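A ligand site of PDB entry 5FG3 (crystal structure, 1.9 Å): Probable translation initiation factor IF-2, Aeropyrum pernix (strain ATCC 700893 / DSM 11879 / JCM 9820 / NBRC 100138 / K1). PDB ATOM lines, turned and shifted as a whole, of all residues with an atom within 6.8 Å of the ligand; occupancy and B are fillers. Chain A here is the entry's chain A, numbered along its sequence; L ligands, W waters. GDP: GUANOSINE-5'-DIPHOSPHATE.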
ATOM      1  N   LEU A  22       5.103  -9.711  -9.900  1.00  0.00           N
ATOM      2  CA  LEU A  22       4.870  -8.735  -8.840  1.00  0.00           C
ATOM      3  C   LEU A  22       5.023  -7.321  -9.375  1.00  0.00           C
ATOM      4  O   LEU A  22       5.442  -7.119 -10.524  1.00  0.00           O
ATOM      5  CB  LEU A  22       5.865  -8.927  -7.701  1.00  0.00           C
ATOM      6  CG  LEU A  22       5.825 -10.281  -6.981  1.00  0.00           C
ATOM      7  CD1 LEU A  22       6.805 -11.235  -7.627  1.00  0.00           C
ATOM      8  CD2 LEU A  22       6.153 -10.155  -5.483  1.00  0.00           C
ATOM      9  N   GLY A  23       4.555  -6.359  -8.584  1.00  0.00           N
ATOM     10  CA  GLY A  23       4.838  -4.945  -8.805  1.00  0.00           C
ATOM     11  C   GLY A  23       3.596  -4.115  -8.519  1.00  0.00           C
ATOM     12  O   GLY A  23       2.522  -4.665  -8.275  1.00  0.00           O
ATOM     13  N   HIS A  24       3.773  -2.801  -8.566  1.00  0.00           N
ATOM     14  CA  HIS A  24       2.723  -1.823  -8.217  1.00  0.00           C
ATOM     15  C   HIS A  24       1.571  -1.827  -9.211  1.00  0.00           C
ATOM     16  O   HIS A  24       1.741  -2.165 -10.397  1.00  0.00           O
ATOM     17  CB  HIS A  24       3.345  -0.406  -8.053  1.00  0.00           C
ATOM     18  CG  HIS A  24       2.432   0.637  -7.470  1.00  0.00           C
ATOM     19  ND1 HIS A  24       2.447   0.951  -6.123  1.00  0.00           N
ATOM     20  CD2 HIS A  24       1.547   1.493  -8.032  1.00  0.00           C
ATOM     21  CE1 HIS A  24       1.575   1.917  -5.884  1.00  0.00           C
ATOM     22  NE2 HIS A  24       1.003   2.260  -7.031  1.00  0.00           N
ATOM     23  N   VAL A  25       0.374  -1.485  -8.706  1.00  0.00           N
ATOM     24  CA  VAL A  25      -0.823  -1.445  -9.527  1.00  0.00           C
ATOM     25  C   VAL A  25      -0.571  -0.590 -10.767  1.00  0.00           C
ATOM     26  O   VAL A  25       0.061   0.473 -10.700  1.00  0.00           O
ATOM     27  CB  VAL A  25      -2.097  -0.973  -8.775  1.00  0.00           C
ATOM     28  CG1 VAL A  25      -1.947   0.442  -8.258  1.00  0.00           C
ATOM     29  CG2 VAL A  25      -3.329  -1.064  -9.677  1.00  0.00           C
ATOM     30  N   ASP A  26      -1.058  -1.098 -11.893  1.00  0.00           N
ATOM     31  CA  ASP A  26      -0.923  -0.495 -13.221  1.00  0.00           C
ATOM     32  C   ASP A  26       0.504  -0.323 -13.779  1.00  0.00           C
ATOM     33  O   ASP A  26       0.687   0.378 -14.728  1.00  0.00           O
ATOM     34  CB  ASP A  26      -1.705   0.829 -13.310  1.00  0.00           C
ATOM     35  CG  ASP A  26      -3.204   0.632 -13.159  1.00  0.00           C
ATOM     36  OD1 ASP A  26      -3.759  -0.441 -13.500  1.00  0.00           O
ATOM     37  OD2 ASP A  26      -3.837   1.604 -12.691  1.00  0.00           O
ATOM     38  N   HIS A  27       1.488  -1.002 -13.219  1.00  0.00           N
ATOM     39  CA  HIS A  27       2.831  -0.979 -13.796  1.00  0.00           C
ATOM     40  C   HIS A  27       2.965  -1.981 -14.961  1.00  0.00           C
ATOM     41  O   HIS A  27       3.910  -1.917 -15.747  1.00  0.00           O
ATOM     42  CB  HIS A  27       3.927  -1.121 -12.701  1.00  0.00           C
ATOM     43  CG  HIS A  27       4.149   0.143 -11.929  1.00  0.00           C
ATOM     44  ND1 HIS A  27       5.285   0.385 -11.180  1.00  0.00           N
ATOM     45  CD2 HIS A  27       3.383   1.257 -11.792  1.00  0.00           C
ATOM     46  CE1 HIS A  27       5.213   1.582 -10.636  1.00  0.00           C
ATOM     47  NE2 HIS A  27       4.066   2.137 -10.990  1.00  0.00           N
ATOM     48  N   GLY A  28       1.966  -2.866 -15.106  1.00  0.00           N
ATOM     49  CA  GLY A  28       1.792  -3.681 -16.303  1.00  0.00           C
ATOM     50  C   GLY A  28       1.961  -5.178 -16.167  1.00  0.00           C
ATOM     51  O   GLY A  28       2.286  -5.844 -17.145  1.00  0.00           O
ATOM     52  N   LYS A  29       1.724  -5.715 -14.972  1.00  0.00           N
ATOM     53  CA  LYS A  29       1.850  -7.140 -14.672  1.00  0.00           C
ATOM     54  C   LYS A  29       0.943  -7.980 -15.583  1.00  0.00           C
ATOM     55  O   LYS A  29       1.382  -8.977 -16.192  1.00  0.00           O
ATOM     56  CB  LYS A  29       1.475  -7.428 -13.217  1.00  0.00           C
ATOM     57  CG  LYS A  29       2.348  -6.757 -12.157  1.00  0.00           C
ATOM     58  CD  LYS A  29       1.904  -7.011 -10.727  1.00  0.00           C
ATOM     59  CE  LYS A  29       0.530  -6.455 -10.380  1.00  0.00           C
ATOM     60  NZ  LYS A  29       0.434  -4.978 -10.450  1.00  0.00           N
ATOM     61  N   THR A  30      -0.315  -7.561 -15.694  1.00  0.00           N
ATOM     62  CA  THR A  30      -1.307  -8.339 -16.429  1.00  0.00           C
ATOM     63  C   THR A  30      -0.990  -8.295 -17.926  1.00  0.00           C
ATOM     64  O   THR A  30      -1.005  -9.335 -18.604  1.00  0.00           O
ATOM     65  CB  THR A  30      -2.732  -7.849 -16.140  1.00  0.00           C
ATOM     66  OG1 THR A  30      -3.017  -8.044 -14.737  1.00  0.00           O
ATOM     67  CG2 THR A  30      -3.771  -8.609 -16.982  1.00  0.00           C
ATOM     68  N   THR A  31      -0.688  -7.099 -18.421  1.00  0.00           N
ATOM     69  CA  THR A  31      -0.355  -6.915 -19.836  1.00  0.00           C
ATOM     70  C   THR A  31       0.884  -7.745 -20.192  1.00  0.00           C
ATOM     71  O   THR A  31       0.929  -8.394 -21.247  1.00  0.00           O
ATOM     72  CB  THR A  31      -0.201  -5.433 -20.170  1.00  0.00           C
ATOM     73  OG1 THR A  31      -1.401  -4.756 -19.808  1.00  0.00           O
ATOM     74  CG2 THR A  31       0.026  -5.205 -21.649  1.00  0.00           C
ATOM     75  N   LEU A  32       1.874  -7.727 -19.310  1.00  0.00           N
ATOM     76  CA  LEU A  32       3.096  -8.500 -19.523  1.00  0.00           C
ATOM     77  C   LEU A  32       2.878 -10.015 -19.568  1.00  0.00           C
ATOM     78  O   LEU A  32       3.469 -10.695 -20.450  1.00  0.00           O
ATOM     79  CB  LEU A  32       4.149  -8.163 -18.458  1.00  0.00           C
ATOM     80  CG  LEU A  32       5.514  -8.856 -18.628  1.00  0.00           C
ATOM     81  CD1 LEU A  32       6.080  -8.527 -20.012  1.00  0.00           C
ATOM     82  CD2 LEU A  32       6.502  -8.472 -17.528  1.00  0.00           C
ATOM     83  N   PRO A  89      -1.570 -12.188 -11.264  1.00  0.00           N
ATOM     84  CA  PRO A  89      -0.387 -11.471 -10.749  1.00  0.00           C
ATOM     85  C   PRO A  89      -0.583 -10.893  -9.338  1.00  0.00           C
ATOM     86  O   PRO A  89      -1.656 -10.972  -8.796  1.00  0.00           O
ATOM     87  CB  PRO A  89      -0.226 -10.364 -11.770  1.00  0.00           C
ATOM     88  CG  PRO A  89      -1.637 -10.023 -12.115  1.00  0.00           C
ATOM     89  CD  PRO A  89      -2.472 -11.272 -11.975  1.00  0.00           C
ATOM     90  N   VAL A 111       7.841  -6.175 -11.838  1.00  0.00           N
ATOM     91  CA  VAL A 111       7.573  -5.197 -12.870  1.00  0.00           C
ATOM     92  C   VAL A 111       7.649  -3.800 -12.249  1.00  0.00           C
ATOM     93  O   VAL A 111       7.082  -3.557 -11.195  1.00  0.00           O
ATOM     94  CB  VAL A 111       6.177  -5.392 -13.505  1.00  0.00           C
ATOM     95  CG1 VAL A 111       5.926  -4.344 -14.586  1.00  0.00           C
ATOM     96  CG2 VAL A 111       6.003  -6.826 -14.041  1.00  0.00           C
ATOM     97  N   ASP A 113       7.176   0.243 -13.719  1.00  0.00           N
ATOM     98  CA  ASP A 113       6.902   1.165 -14.792  1.00  0.00           C
ATOM     99  C   ASP A 113       8.118   2.107 -14.926  1.00  0.00           C
ATOM    100  O   ASP A 113       8.354   2.914 -14.023  1.00  0.00           O
ATOM    101  CB  ASP A 113       5.631   1.954 -14.445  1.00  0.00           C
ATOM    102  CG  ASP A 113       5.230   2.992 -15.529  1.00  0.00           C
ATOM    103  OD1 ASP A 113       6.007   3.341 -16.423  1.00  0.00           O
ATOM    104  OD2 ASP A 113       4.085   3.471 -15.455  1.00  0.00           O
ATOM    105  N   ASN A 141       9.268  -1.824 -17.343  1.00  0.00           N
ATOM    106  CA  ASN A 141       8.235  -1.858 -18.334  1.00  0.00           C
ATOM    107  C   ASN A 141       7.797  -0.477 -18.849  1.00  0.00           C
ATOM    108  O   ASN A 141       8.098   0.549 -18.256  1.00  0.00           O
ATOM    109  CB  ASN A 141       7.055  -2.639 -17.738  1.00  0.00           C
ATOM    110  CG  ASN A 141       6.002  -2.991 -18.773  1.00  0.00           C
ATOM    111  OD1 ASN A 141       6.327  -3.370 -19.917  1.00  0.00           O
ATOM    112  ND2 ASN A 141       4.726  -2.840 -18.397  1.00  0.00           N
ATOM    113  N   LYS A 142       7.132  -0.516 -20.009  1.00  0.00           N
ATOM    114  CA  LYS A 142       6.547   0.631 -20.691  1.00  0.00           C
ATOM    115  C   LYS A 142       7.626   1.527 -21.360  1.00  0.00           C
ATOM    116  O   LYS A 142       7.429   2.736 -21.480  1.00  0.00           O
ATOM    117  CB  LYS A 142       5.604   1.444 -19.800  1.00  0.00           C
ATOM    118  CG  LYS A 142       4.644   0.649 -18.895  1.00  0.00           C
ATOM    119  CD  LYS A 142       3.414   1.485 -18.519  1.00  0.00           C
ATOM    120  CE  LYS A 142       2.568   0.792 -17.468  1.00  0.00           C
ATOM    121  NZ  LYS A 142       1.468   1.666 -16.968  1.00  0.00           N
ATOM    122  N   ILE A 143       8.713   0.931 -21.825  1.00  0.00           N
ATOM    123  CA  ILE A 143       9.760   1.710 -22.544  1.00  0.00           C
ATOM    124  C   ILE A 143       9.250   2.439 -23.759  1.00  0.00           C
ATOM    125  O   ILE A 143       9.782   3.495 -24.128  1.00  0.00           O
ATOM    126  CB  ILE A 143      10.971   0.848 -22.979  1.00  0.00           C
ATOM    127  CG1 ILE A 143      10.550  -0.269 -23.969  1.00  0.00           C
ATOM    128  CG2 ILE A 143      11.679   0.287 -21.742  1.00  0.00           C
ATOM    129  CD1 ILE A 143      11.652  -1.274 -24.231  1.00  0.00           C
ATOM    130  N   ASP A 144       8.216   1.883 -24.398  1.00  0.00           N
ATOM    131  CA  ASP A 144       7.534   2.525 -25.515  1.00  0.00           C
ATOM    132  C   ASP A 144       6.870   3.835 -25.199  1.00  0.00           C
ATOM    133  O   ASP A 144       6.525   4.569 -26.121  1.00  0.00           O
ATOM    134  CB  ASP A 144       6.460   1.587 -26.088  1.00  0.00           C
ATOM    135  CG  ASP A 144       5.341   1.350 -25.106  1.00  0.00           C
ATOM    136  OD1 ASP A 144       5.566   0.589 -24.138  1.00  0.00           O
ATOM    137  OD2 ASP A 144       4.257   1.947 -25.262  1.00  0.00           O
ATOM    138  N   ARG A 145       6.646   4.134 -23.922  1.00  0.00           N
ATOM    139  CA  ARG A 145       6.115   5.446 -23.513  1.00  0.00           C
ATOM    140  C   ARG A 145       7.186   6.539 -23.367  1.00  0.00           C
ATOM    141  O   ARG A 145       6.850   7.681 -23.061  1.00  0.00           O
ATOM    142  CB  ARG A 145       5.357   5.339 -22.195  1.00  0.00           C
ATOM    143  CG  ARG A 145       3.985   4.703 -22.358  1.00  0.00           C
ATOM    144  CD  ARG A 145       3.279   4.536 -21.045  1.00  0.00           C
ATOM    145  NE  ARG A 145       3.013   5.825 -20.429  1.00  0.00           N
ATOM    146  CZ  ARG A 145       2.036   6.658 -20.797  1.00  0.00           C
ATOM    147  NH1 ARG A 145       1.209   6.352 -21.793  1.00  0.00           N
ATOM    148  NH2 ARG A 145       1.909   7.815 -20.160  1.00  0.00           N
ATOM    149  N   VAL A 208      11.625  -3.497 -21.103  1.00  0.00           N
ATOM    150  CA  VAL A 208      10.641  -4.211 -21.927  1.00  0.00           C
ATOM    151  C   VAL A 208       9.434  -3.306 -22.172  1.00  0.00           C
ATOM    152  O   VAL A 208       9.298  -2.275 -21.527  1.00  0.00           O
ATOM    153  CB  VAL A 208      10.130  -5.542 -21.293  1.00  0.00           C
ATOM    154  CG1 VAL A 208      11.271  -6.556 -21.057  1.00  0.00           C
ATOM    155  CG2 VAL A 208       9.333  -5.298 -20.008  1.00  0.00           C
ATOM    156  N   SER A 209       8.602  -3.711 -23.119  1.00  0.00           N
ATOM    157  CA  SER A 209       7.271  -3.136 -23.344  1.00  0.00           C
ATOM    158  C   SER A 209       6.323  -4.309 -23.457  1.00  0.00           C
ATOM    159  O   SER A 209       6.343  -5.079 -24.413  1.00  0.00           O
ATOM    160  CB  SER A 209       7.224  -2.272 -24.619  1.00  0.00           C
ATOM    161  OG  SER A 209       5.861  -1.844 -24.845  1.00  0.00           O
ATOM    162  N   ALA A 210       5.503  -4.479 -22.428  1.00  0.00           N
ATOM    163  CA  ALA A 210       4.404  -5.442 -22.470  1.00  0.00           C
ATOM    164  C   ALA A 210       3.446  -5.126 -23.629  1.00  0.00           C
ATOM    165  O   ALA A 210       2.775  -6.039 -24.132  1.00  0.00           O
ATOM    166  CB  ALA A 210       3.655  -5.423 -21.161  1.00  0.00           C
ATOM    167  N   ARG A 211       3.399  -3.875 -24.076  1.00  0.00           N
ATOM    168  CA  ARG A 211       2.556  -3.490 -25.190  1.00  0.00           C
ATOM    169  C   ARG A 211       3.118  -3.849 -26.586  1.00  0.00           C
ATOM    170  O   ARG A 211       2.389  -4.370 -27.419  1.00  0.00           O
ATOM    171  CB  ARG A 211       2.242  -1.998 -25.119  1.00  0.00           C
ATOM    172  CG  ARG A 211       1.411  -1.507 -26.281  1.00  0.00           C
ATOM    173  CD  ARG A 211       0.782  -0.149 -26.047  1.00  0.00           C
ATOM    174  NE  ARG A 211      -0.209  -0.164 -24.977  1.00  0.00           N
ATOM    175  CZ  ARG A 211      -1.255   0.661 -24.881  1.00  0.00           C
ATOM    176  NH1 ARG A 211      -1.525   1.553 -25.824  1.00  0.00           N
ATOM    177  NH2 ARG A 211      -2.069   0.562 -23.831  1.00  0.00           N
ATOM    178  N   THR A 212       4.391  -3.547 -26.864  1.00  0.00           N
ATOM    179  CA  THR A 212       4.954  -3.751 -28.197  1.00  0.00           C
ATOM    180  C   THR A 212       5.721  -5.050 -28.317  1.00  0.00           C
ATOM    181  O   THR A 212       6.112  -5.414 -29.424  1.00  0.00           O
ATOM    182  CB  THR A 212       5.972  -2.633 -28.589  1.00  0.00           C
ATOM    183  OG1 THR A 212       7.167  -2.814 -27.850  1.00  0.00           O
ATOM    184  CG2 THR A 212       5.413  -1.232 -28.287  1.00  0.00           C
ATOM    185  N   GLY A 213       6.003  -5.718 -27.200  1.00  0.00           N
ATOM    186  CA  GLY A 213       6.882  -6.914 -27.224  1.00  0.00           C
ATOM    187  C   GLY A 213       8.384  -6.698 -27.215  1.00  0.00           C
ATOM    188  O   GLY A 213       9.145  -7.693 -27.199  1.00  0.00           O
HETATM  189  PB  GDP L   1      -1.277  -4.245 -13.517  1.00  0.00           P
HETATM  190  O1B GDP L   1      -2.263  -3.476 -12.704  1.00  0.00           O
HETATM  191  O2B GDP L   1      -1.615  -5.676 -13.805  1.00  0.00           O
HETATM  192  O3B GDP L   1       0.155  -4.143 -13.026  1.00  0.00           O
HETATM  193  O3A GDP L   1      -1.187  -3.375 -14.889  1.00  0.00           O
HETATM  194  PA  GDP L   1      -1.997  -3.699 -16.226  1.00  0.00           P
HETATM  195  O1A GDP L   1      -1.321  -4.842 -16.970  1.00  0.00           O
HETATM  196  O2A GDP L   1      -3.466  -3.773 -15.954  1.00  0.00           O
HETATM  197  O5' GDP L   1      -1.701  -2.406 -17.110  1.00  0.00           O
HETATM  198  C5' GDP L   1      -2.067  -1.085 -16.689  1.00  0.00           C
HETATM  199  C4' GDP L   1      -2.255  -0.161 -17.876  1.00  0.00           C
HETATM  200  O4' GDP L   1      -0.978   0.109 -18.455  1.00  0.00           O
HETATM  201  C3' GDP L   1      -3.150  -0.715 -18.993  1.00  0.00           C
HETATM  202  O3' GDP L   1      -3.832   0.361 -19.652  1.00  0.00           O
HETATM  203  C2' GDP L   1      -2.143  -1.313 -19.934  1.00  0.00           C
HETATM  204  O2' GDP L   1      -2.598  -1.359 -21.274  1.00  0.00           O
HETATM  205  C1' GDP L   1      -0.988  -0.334 -19.794  1.00  0.00           C
HETATM  206  N9  GDP L   1       0.319  -0.949 -20.099  1.00  0.00           N
HETATM  207  C8  GDP L   1       0.849  -2.069 -19.564  1.00  0.00           C
HETATM  208  N7  GDP L   1       2.081  -2.313 -20.110  1.00  0.00           N
HETATM  209  C5  GDP L   1       2.354  -1.330 -20.988  1.00  0.00           C
HETATM  210  C6  GDP L   1       3.473  -0.966 -21.878  1.00  0.00           C
HETATM  211  O6  GDP L   1       4.551  -1.644 -21.983  1.00  0.00           O
HETATM  212  N1  GDP L   1       3.317   0.141 -22.583  1.00  0.00           N
HETATM  213  C2  GDP L   1       2.217   0.935 -22.515  1.00  0.00           C
HETATM  214  N2  GDP L   1       2.149   2.028 -23.274  1.00  0.00           N
HETATM  215  N3  GDP L   1       1.157   0.667 -21.726  1.00  0.00           N
HETATM  216  C4  GDP L   1       1.189  -0.431 -20.955  1.00  0.00           C
HETATM  217  O   HOH W   1      -6.097  -0.688 -20.859  1.00  0.00           O
HETATM  218  O   HOH W   2      -5.534  -5.090 -13.571  1.00  0.00           O
HETATM  219  O   HOH W   3      -2.216  -4.616  -9.912  1.00  0.00           O
HETATM  220  O   HOH W   4      -4.433  -2.812 -13.667  1.00  0.00           O
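His 24 touches the ligand. Val 25 touches the ligand. CG of Arg 145 touches N2 of the ligand, at 3.4 Å. Within 4 Å of the ligand: His 24, Val 25, Asp 26, His 27, Gly 28, Lys 29, Thr 30, Thr 31, Asn 141, Lys 142, Asp 144, Arg 145, Ser 209, Ala 210 and Arg 211. The nearest printed residue that does not touch the ligand is Pro 89 (4.7 Å).
Water W4 bridges an oxygen (O1B) of the ligand and the side-chain carboxylate (OD1) of Asp 26. Water W3 lies within hydrogen-bond range of the side-chain amino group (NZ) of Lys 29 (2.7 Å) and an oxygen (O1B) of the ligand (3.0 Å).
N of Lys 142 lies within hydrogen-bond range of O of Val 208. The side-chain hydroxyl (OG) of Ser 209 sits at hydrogen-bond distance from the side-chain carboxylate (OD1) of Asp 144 (2.6 Å). ND2 of Asn 141 is in hydrogen-bond range of O of His 27 (2.9 Å). The side-chain hydroxyl of Ser 209 lies close to the backbone NH of Arg 211. ND1 of His 27 sits at hydrogen-bond distance from N of Asp 113 (3.2 Å). The backbone carbonyl oxygen (O) of Asp 26 lies within hydrogen-bond range of the side-chain amino group (NZ) of Lys 142, 2.7 Å away. NZ of Lys 29 sits at hydrogen-bond distance from O of Gly 23 (3.0 Å). The side-chain carboxylate of Asp 113 lies within salt-bridge range of the side-chain amino group of Lys 142.
The side-chain hydroxyl (OG) of Ser 209 lies within hydrogen-bond range of an oxygen (O6) of the ligand, 3.2 Å away. The side-chain amide nitrogen (ND2) of Asn 141 sits at hydrogen-bond distance from a nitrogen (N7) of the ligand (3.2 Å). An oxygen (O1A) of the ligand sits at hydrogen-bond distance from the backbone NH (N) of Thr 31 (2.8 Å). The backbone NH of Asp 26 lies within hydrogen-bond range of an oxygen (O1B) of the ligand (2.8 Å). NH2 of Arg 211 sits at hydrogen-bond distance from O2' of the ligand (3.2 Å). N of Lys 142 sits close to O6 of the ligand. An oxygen (O3B) of the ligand lies within salt-bridge range of the side-chain amino group of Lys 29, 2.7 Å away. The side-chain hydroxyl (OG1) of Thr 30 is in hydrogen-bond range of an oxygen (O2B) of the ligand (2.9 Å). O3B of the ligand lies within hydrogen-bond range of N of Lys 29. N1 of the ligand lies within hydrogen-bond range of OD1 of Asp 144, at 2.8 Å. The backbone NH (N) of Ala 210 lies within hydrogen-bond range of an oxygen (O6) of the ligand, at 3.0 Å. The backbone NH (N) of Gly 28 lies within hydrogen-bond range of an oxygen (O3B) of the ligand, at 3.0 Å. An oxygen (O2B) of the ligand is in hydrogen-bond range of the backbone NH of Thr 30 (3.0 Å). The backbone NH of Arg 211 sits at hydrogen-bond distance from an oxygen (O6) of the ligand (3.3 Å). N of His 27 is in hydrogen-bond range of O3B of the ligand (3.4 Å). The side-chain amino group (NZ) of Lys 142 sits at hydrogen-bond distance from an oxygen (O4') of the ligand. An oxygen (O1A) of the ligand is in hydrogen-bond range of the side-chain hydroxyl (OG1) of Thr 31 (2.8 Å).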
